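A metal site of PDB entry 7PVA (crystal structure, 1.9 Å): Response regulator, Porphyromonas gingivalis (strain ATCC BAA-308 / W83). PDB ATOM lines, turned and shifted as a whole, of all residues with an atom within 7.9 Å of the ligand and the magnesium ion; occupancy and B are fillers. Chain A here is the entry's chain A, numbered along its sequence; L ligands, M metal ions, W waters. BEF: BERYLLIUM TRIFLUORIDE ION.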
ATOM      1  N   ALA A  18      -0.523  21.855  28.491  1.00  0.00           N
ATOM      2  CA  ALA A  18       0.436  22.632  27.731  1.00  0.00           C
ATOM      3  C   ALA A  18       0.167  22.443  26.253  1.00  0.00           C
ATOM      4  O   ALA A  18       0.234  21.316  25.761  1.00  0.00           O
ATOM      5  CB  ALA A  18       1.872  22.223  28.086  1.00  0.00           C
ATOM      6  N   ASP A  19      -0.105  23.532  25.531  1.00  0.00           N
ATOM      7  CA  ASP A  19      -0.247  23.567  24.075  1.00  0.00           C
ATOM      8  C   ASP A  19      -0.023  25.016  23.650  1.00  0.00           C
ATOM      9  O   ASP A  19      -0.612  25.936  24.215  1.00  0.00           O
ATOM     10  CB  ASP A  19      -1.628  23.099  23.642  1.00  0.00           C
ATOM     11  CG  ASP A  19      -1.698  22.725  22.176  1.00  0.00           C
ATOM     12  OD1 ASP A  19      -1.525  23.622  21.336  1.00  0.00           O
ATOM     13  OD2 ASP A  19      -2.003  21.559  21.839  1.00  0.00           O
ATOM     14  N   ASP A  20       0.801  25.213  22.620  1.00  0.00           N
ATOM     15  CA  ASP A  20       0.992  26.566  22.082  1.00  0.00           C
ATOM     16  C   ASP A  20      -0.238  27.103  21.368  1.00  0.00           C
ATOM     17  O   ASP A  20      -0.275  28.293  21.066  1.00  0.00           O
ATOM     18  CB  ASP A  20       2.189  26.598  21.121  1.00  0.00           C
ATOM     19  CG  ASP A  20       2.067  25.585  19.963  1.00  0.00           C
ATOM     20  OD1 ASP A  20       1.669  24.401  20.143  1.00  0.00           O
ATOM     21  OD2 ASP A  20       2.402  25.976  18.842  1.00  0.00           O
ATOM     22  N   GLU A  21      -1.215  26.276  21.044  1.00  0.00           N
ATOM     23  CA  GLU A  21      -2.443  26.675  20.360  1.00  0.00           C
ATOM     24  C   GLU A  21      -3.649  26.421  21.274  1.00  0.00           C
ATOM     25  O   GLU A  21      -4.702  25.964  20.850  1.00  0.00           O
ATOM     26  CB  GLU A  21      -2.590  25.931  19.043  1.00  0.00           C
ATOM     27  CG  GLU A  21      -1.521  26.258  18.008  1.00  0.00           C
ATOM     28  CD  GLU A  21      -1.679  25.448  16.766  1.00  0.00           C
ATOM     29  OE1 GLU A  21      -1.671  24.196  16.844  1.00  0.00           O
ATOM     30  OE2 GLU A  21      -1.812  26.070  15.686  1.00  0.00           O
ATOM     31  N   ILE A  22      -3.474  26.684  22.567  1.00  0.00           N
ATOM     32  CA  ILE A  22      -4.500  26.385  23.563  1.00  0.00           C
ATOM     33  C   ILE A  22      -5.803  27.127  23.249  1.00  0.00           C
ATOM     34  O   ILE A  22      -6.884  26.705  23.672  1.00  0.00           O
ATOM     35  CB  ILE A  22      -3.941  26.754  24.963  1.00  0.00           C
ATOM     36  CG1 ILE A  22      -4.680  26.043  26.094  1.00  0.00           C
ATOM     37  CG2 ILE A  22      -4.017  28.288  25.174  1.00  0.00           C
ATOM     38  CD1 ILE A  22      -4.435  24.620  26.138  1.00  0.00           C
ATOM     39  N   LEU A  25      -8.244  24.942  21.829  1.00  0.00           N
ATOM     40  CA  LEU A  25      -8.713  23.929  22.721  1.00  0.00           C
ATOM     41  C   LEU A  25      -9.752  24.452  23.680  1.00  0.00           C
ATOM     42  O   LEU A  25     -10.201  23.703  24.571  1.00  0.00           O
ATOM     43  CB  LEU A  25      -7.493  23.441  23.432  1.00  0.00           C
ATOM     44  CG  LEU A  25      -6.905  22.104  22.990  1.00  0.00           C
ATOM     45  CD1 LEU A  25      -7.196  21.244  21.676  1.00  0.00           C
ATOM     46  CD2 LEU A  25      -5.231  22.283  22.935  1.00  0.00           C
ATOM     47  N   LEU A  43       1.530  27.585  27.720  1.00  0.00           N
ATOM     48  CA  LEU A  43       1.762  27.650  26.279  1.00  0.00           C
ATOM     49  C   LEU A  43       3.042  26.982  25.796  1.00  0.00           C
ATOM     50  O   LEU A  43       3.305  26.942  24.584  1.00  0.00           O
ATOM     51  CB  LEU A  43       1.767  29.104  25.803  1.00  0.00           C
ATOM     52  CG  LEU A  43       0.470  29.874  26.040  1.00  0.00           C
ATOM     53  CD1 LEU A  43       0.774  31.375  25.853  1.00  0.00           C
ATOM     54  CD2 LEU A  43      -0.638  29.359  25.134  1.00  0.00           C
ATOM     55  N   LEU A  62      -0.123  17.169  27.305  1.00  0.00           N
ATOM     56  CA  LEU A  62       0.994  17.785  26.596  1.00  0.00           C
ATOM     57  C   LEU A  62       0.838  17.730  25.083  1.00  0.00           C
ATOM     58  O   LEU A  62       0.780  16.644  24.501  1.00  0.00           O
ATOM     59  CB  LEU A  62       2.306  17.064  26.950  1.00  0.00           C
ATOM     60  CG  LEU A  62       3.076  17.260  28.237  1.00  0.00           C
ATOM     61  CD1 LEU A  62       4.377  16.492  28.084  1.00  0.00           C
ATOM     62  CD2 LEU A  62       3.327  18.721  28.497  1.00  0.00           C
ATOM     63  N   ASP A  63       1.020  18.875  24.432  1.00  0.00           N
ATOM     64  CA  ASP A  63       1.313  18.984  23.006  1.00  0.00           C
ATOM     65  C   ASP A  63       2.727  18.509  22.710  1.00  0.00           C
ATOM     66  O   ASP A  63       3.574  18.488  23.590  1.00  0.00           O
ATOM     67  CB  ASP A  63       1.137  20.440  22.603  1.00  0.00           C
ATOM     68  CG  ASP A  63       1.176  20.691  21.109  1.00  0.00           C
ATOM     69  OD1 ASP A  63       0.899  19.797  20.267  1.00  0.00           O
ATOM     70  OD2 ASP A  63       1.472  21.871  20.812  1.00  0.00           O
ATOM     71  N   GLU A  64       2.991  18.161  21.431  1.00  0.00           N
ATOM     72  CA  GLU A  64       4.333  17.775  21.035  1.00  0.00           C
ATOM     73  C   GLU A  64       5.089  18.985  20.459  1.00  0.00           C
ATOM     74  O   GLU A  64       6.165  19.361  20.958  1.00  0.00           O
ATOM     75  CB  GLU A  64       4.297  16.597  20.038  1.00  0.00           C
ATOM     76  CG  GLU A  64       5.723  16.046  19.761  1.00  0.00           C
ATOM     77  CD  GLU A  64       6.498  16.831  18.695  1.00  0.00           C
ATOM     78  OE1 GLU A  64       5.888  17.285  17.690  1.00  0.00           O
ATOM     79  OE2 GLU A  64       7.729  16.912  18.844  1.00  0.00           O
ATOM     80  N   ASN A  65       4.505  19.647  19.477  1.00  0.00           N
ATOM     81  CA  ASN A  65       5.206  20.704  18.744  1.00  0.00           C
ATOM     82  C   ASN A  65       4.876  22.059  19.346  1.00  0.00           C
ATOM     83  O   ASN A  65       3.774  22.578  19.137  1.00  0.00           O
ATOM     84  CB  ASN A  65       4.838  20.699  17.265  1.00  0.00           C
ATOM     85  CG  ASN A  65       5.655  21.685  16.427  1.00  0.00           C
ATOM     86  OD1 ASN A  65       6.314  22.531  16.937  1.00  0.00           O
ATOM     87  ND2 ASN A  65       5.595  21.559  15.151  1.00  0.00           N
ATOM     88  N   MET A  66       5.818  22.622  20.088  1.00  0.00           N
ATOM     89  CA  MET A  66       5.706  23.888  20.780  1.00  0.00           C
ATOM     90  C   MET A  66       7.037  24.641  20.562  1.00  0.00           C
ATOM     91  O   MET A  66       8.085  24.056  20.626  1.00  0.00           O
ATOM     92  CB  MET A  66       5.466  23.686  22.301  1.00  0.00           C
ATOM     93  CG  MET A  66       4.054  23.325  22.593  1.00  0.00           C
ATOM     94  SD  MET A  66       3.720  22.956  24.413  1.00  0.00           S
ATOM     95  CE  MET A  66       4.994  21.530  24.725  1.00  0.00           C
ATOM     96  N   PRO A  67       6.979  25.946  20.356  1.00  0.00           N
ATOM     97  CA  PRO A  67       8.217  26.727  20.383  1.00  0.00           C
ATOM     98  C   PRO A  67       8.932  26.531  21.723  1.00  0.00           C
ATOM     99  O   PRO A  67       8.340  26.640  22.791  1.00  0.00           O
ATOM    100  CB  PRO A  67       7.735  28.178  20.184  1.00  0.00           C
ATOM    101  CG  PRO A  67       6.332  28.029  19.582  1.00  0.00           C
ATOM    102  CD  PRO A  67       5.779  26.800  20.208  1.00  0.00           C
ATOM    103  N   GLY A  71       7.340  18.781  23.421  1.00  0.00           N
ATOM    104  CA  GLY A  71       6.578  18.042  24.417  1.00  0.00           C
ATOM    105  C   GLY A  71       7.309  16.803  24.888  1.00  0.00           C
ATOM    106  O   GLY A  71       7.187  16.393  26.052  1.00  0.00           O
ATOM    107  N   MET A  89      -0.323  12.667  25.974  1.00  0.00           N
ATOM    108  CA  MET A  89       0.146  13.476  24.854  1.00  0.00           C
ATOM    109  C   MET A  89      -1.018  13.693  23.910  1.00  0.00           C
ATOM    110  O   MET A  89      -1.670  12.721  23.556  1.00  0.00           O
ATOM    111  CB  MET A  89       1.346  12.800  24.144  1.00  0.00           C
ATOM    112  CG  MET A  89       1.752  13.620  22.902  1.00  0.00           C
ATOM    113  SD  MET A  89       3.666  13.469  22.470  1.00  0.00           S
ATOM    114  CE  MET A  89       4.170  14.672  23.937  1.00  0.00           C
ATOM    115  N   ILE A  90      -1.290  14.960  23.559  1.00  0.00           N
ATOM    116  CA  ILE A  90      -2.391  15.334  22.658  1.00  0.00           C
ATOM    117  C   ILE A  90      -1.765  16.137  21.544  1.00  0.00           C
ATOM    118  O   ILE A  90      -1.325  17.277  21.740  1.00  0.00           O
ATOM    119  CB  ILE A  90      -3.490  16.114  23.390  1.00  0.00           C
ATOM    120  CG1 ILE A  90      -4.076  15.178  24.490  1.00  0.00           C
ATOM    121  CG2 ILE A  90      -4.617  16.554  22.395  1.00  0.00           C
ATOM    122  CD1 ILE A  90      -4.978  15.912  25.496  1.00  0.00           C
ATOM    123  N   THR A  91      -1.632  15.506  20.381  1.00  0.00           N
ATOM    124  CA  THR A  91      -0.838  16.088  19.322  1.00  0.00           C
ATOM    125  C   THR A  91      -1.482  15.919  17.943  1.00  0.00           C
ATOM    126  O   THR A  91      -2.200  14.946  17.668  1.00  0.00           O
ATOM    127  CB  THR A  91       0.560  15.488  19.365  1.00  0.00           C
ATOM    128  OG1 THR A  91       1.312  16.002  18.269  1.00  0.00           O
ATOM    129  CG2 THR A  91       0.452  14.036  19.219  1.00  0.00           C
ATOM    130  N   LYS A  92      -1.151  16.864  17.034  1.00  0.00           N
ATOM    131  CA  LYS A  92      -1.558  16.649  15.656  1.00  0.00           C
ATOM    132  C   LYS A  92      -0.672  15.663  14.900  1.00  0.00           C
ATOM    133  O   LYS A  92      -1.034  15.283  13.789  1.00  0.00           O
ATOM    134  CB  LYS A  92      -1.574  17.962  14.881  1.00  0.00           C
ATOM    135  CG  LYS A  92      -0.251  18.667  14.808  1.00  0.00           C
ATOM    136  CD  LYS A  92      -0.325  20.070  14.136  1.00  0.00           C
ATOM    137  CE  LYS A  92      -1.137  21.061  14.991  1.00  0.00           C
ATOM    138  NZ  LYS A  92      -0.645  22.449  14.861  1.00  0.00           N
ATOM    139  N   SER A  93       0.485  15.281  15.448  1.00  0.00           N
ATOM    140  CA  SER A  93       1.445  14.486  14.699  1.00  0.00           C
ATOM    141  C   SER A  93       0.948  13.068  14.551  1.00  0.00           C
ATOM    142  O   SER A  93       0.533  12.437  15.519  1.00  0.00           O
ATOM    143  CB  SER A  93       2.793  14.447  15.415  1.00  0.00           C
ATOM    144  OG  SER A  93       3.579  13.459  14.752  1.00  0.00           O
ATOM    145  N   ILE A  98       7.230   9.642  16.574  1.00  0.00           N
ATOM    146  CA  ILE A  98       6.799  10.438  17.706  1.00  0.00           C
ATOM    147  C   ILE A  98       6.032   9.554  18.669  1.00  0.00           C
ATOM    148  O   ILE A  98       6.162   9.645  19.885  1.00  0.00           O
ATOM    149  CB  ILE A  98       5.979  11.655  17.240  1.00  0.00           C
ATOM    150  CG1 ILE A  98       6.854  12.597  16.362  1.00  0.00           C
ATOM    151  CG2 ILE A  98       5.387  12.474  18.435  1.00  0.00           C
ATOM    152  CD1 ILE A  98       8.129  13.103  17.046  1.00  0.00           C
ATOM    153  N   TYR A 110      -2.114   8.750  24.370  1.00  0.00           N
ATOM    154  CA  TYR A 110      -1.617   9.495  23.229  1.00  0.00           C
ATOM    155  C   TYR A 110      -2.818   9.636  22.336  1.00  0.00           C
ATOM    156  O   TYR A 110      -3.265   8.597  21.843  1.00  0.00           O
ATOM    157  CB  TYR A 110      -0.510   8.746  22.534  1.00  0.00           C
ATOM    158  CG  TYR A 110       0.197   9.464  21.405  1.00  0.00           C
ATOM    159  CD1 TYR A 110      -0.413   9.634  20.147  1.00  0.00           C
ATOM    160  CD2 TYR A 110       1.487   9.912  21.570  1.00  0.00           C
ATOM    161  CE1 TYR A 110       0.262  10.231  19.100  1.00  0.00           C
ATOM    162  CE2 TYR A 110       2.193  10.496  20.532  1.00  0.00           C
ATOM    163  CZ  TYR A 110       1.612  10.620  19.281  1.00  0.00           C
ATOM    164  OH  TYR A 110       2.307  11.264  18.239  1.00  0.00           O
ATOM    165  N   LEU A 111      -3.297  10.860  22.145  1.00  0.00           N
ATOM    166  CA  LEU A 111      -4.489  11.175  21.353  1.00  0.00           C
ATOM    167  C   LEU A 111      -4.097  12.061  20.177  1.00  0.00           C
ATOM    168  O   LEU A 111      -3.511  13.158  20.363  1.00  0.00           O
ATOM    169  CB  LEU A 111      -5.569  11.853  22.205  1.00  0.00           C
ATOM    170  CG  LEU A 111      -5.993  11.054  23.459  1.00  0.00           C
ATOM    171  CD1 LEU A 111      -6.898  11.865  24.280  1.00  0.00           C
ATOM    172  CD2 LEU A 111      -6.715   9.789  22.901  1.00  0.00           C
ATOM    173  N   ILE A 112      -4.381  11.594  18.966  1.00  0.00           N
ATOM    174  CA  ILE A 112      -4.131  12.381  17.770  1.00  0.00           C
ATOM    175  C   ILE A 112      -5.264  13.371  17.503  1.00  0.00           C
ATOM    176  O   ILE A 112      -6.430  12.985  17.384  1.00  0.00           O
ATOM    177  CB  ILE A 112      -3.912  11.453  16.576  1.00  0.00           C
ATOM    178  CG1 ILE A 112      -2.777  10.481  16.871  1.00  0.00           C
ATOM    179  CG2 ILE A 112      -3.672  12.304  15.311  1.00  0.00           C
ATOM    180  CD1 ILE A 112      -2.659   9.373  15.810  1.00  0.00           C
ATOM    181  N   LYS A 113      -4.919  14.652  17.331  1.00  0.00           N
ATOM    182  CA  LYS A 113      -5.910  15.667  16.996  1.00  0.00           C
ATOM    183  C   LYS A 113      -6.501  15.460  15.596  1.00  0.00           C
ATOM    184  O   LYS A 113      -5.858  14.942  14.692  1.00  0.00           O
ATOM    185  CB  LYS A 113      -5.275  17.043  17.059  1.00  0.00           C
ATOM    186  CG  LYS A 113      -4.751  17.494  18.391  1.00  0.00           C
ATOM    187  CD  LYS A 113      -3.893  18.735  18.241  1.00  0.00           C
ATOM    188  CE  LYS A 113      -3.491  19.377  19.576  1.00  0.00           C
ATOM    189  NZ  LYS A 113      -2.588  20.599  19.367  1.00  0.00           N
HETATM  190 BE   BEF L   1       1.003  19.730  18.879  1.00  0.00          BE
HETATM  191  F1  BEF L   1       1.604  20.909  18.106  1.00  0.00           F
HETATM  192  F2  BEF L   1      -0.310  19.329  18.174  1.00  0.00           F
HETATM  193  F3  BEF L   1       1.906  18.575  18.552  1.00  0.00           F
HETATM  194 MG    MG M   1       1.607  22.693  18.963  1.00  0.00          MG
HETATM  195  O   HOH W   1       1.870  23.713  17.162  1.00  0.00           O
HETATM  196  O   HOH W   2       3.461  17.698  16.184  1.00  0.00           O
HETATM  197  O   HOH W   3      -0.407  22.801  18.919  1.00  0.00           O
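N of Asn 65 is in hydrogen-bond range of F3 of the ligand. The side-chain carboxylate of Asp 63 is bound to a beryllium atom (BE) of the ligand. NZ of Lys 113 lies within hydrogen-bond range of F2 of the ligand, 2.9 Å away. F2 of the ligand lies within hydrogen-bond range of N of Lys 92. The side-chain hydroxyl (OG1) of Thr 91 is in hydrogen-bond range of a fluorine (F3) of the ligand, at 2.7 Å. The backbone NH (N) of Glu 64 is in hydrogen-bond range of a fluorine (F3) of the ligand (3.1 Å).
The side-chain carboxylate (OD1) of Asp 63 sits close to the side-chain amino group (NZ) of Lys 113, at 3.7 Å. The backbone carbonyl oxygen (O) of Glu 64 is in hydrogen-bond range of the backbone NH (N) of Gly 71, 2.8 Å away. O of Leu 111 is in hydrogen-bond range of N of Thr 91 (3.0 Å). The backbone carbonyl oxygen (O) of Ala 18 is in hydrogen-bond range of the backbone NH (N) of Asp 63 (2.9 Å). The side-chain amino group (NZ) of Lys 113 lies within salt-bridge range of the side-chain carboxylate (OD2) of Asp 19 (2.7 Å). The side-chain hydroxyl (OG1) of Thr 91 sits at hydrogen-bond distance from the backbone NH (N) of Ser 93, at 3.0 Å. The backbone carbonyl oxygen of Thr 91 is in hydrogen-bond range of the backbone NH of Lys 113 (2.8 Å). The side-chain amino group (NZ) of Lys 92 is in salt-bridge range of the side-chain carboxylate (OE1) of Glu 21 (2.8 Å).
Of the 24 residues printed, 6 come within 4 Å of the ligand.
Within 4 Å of the magnesium ion: Asp 20, Asp 63 and Asn 65. The nearest printed residue that does not touch the magnesium ion is Asp 19 (4.04 Å).
The magnesium ion is bound by a fluorine (F1) of the ligand (2.0 Å), water W3 (2.0 Å), the side-chain carboxylate of Asp 63 (2.0 Å), the side-chain carboxylate of Asp 20 (2.1 Å), water W1 (2.1 Å) and the backbone carbonyl oxygen of Asn 65 (2.2 Å). The magnesium ion has six donor atoms within binding distance.
Water W3 lies within hydrogen-bond range of OD1 of Asp 19 (2.8 Å), OE1 of Glu 21 (2.8 Å) and NZ of Lys 113 (3.1 Å). Water W2 lies within hydrogen-bond range of the side-chain carboxylate of Glu 64 (2.9 Å), a fluorine (F3) of the ligand (3.0 Å) and the side-chain hydroxyl of Thr 91 (3.4 Å).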
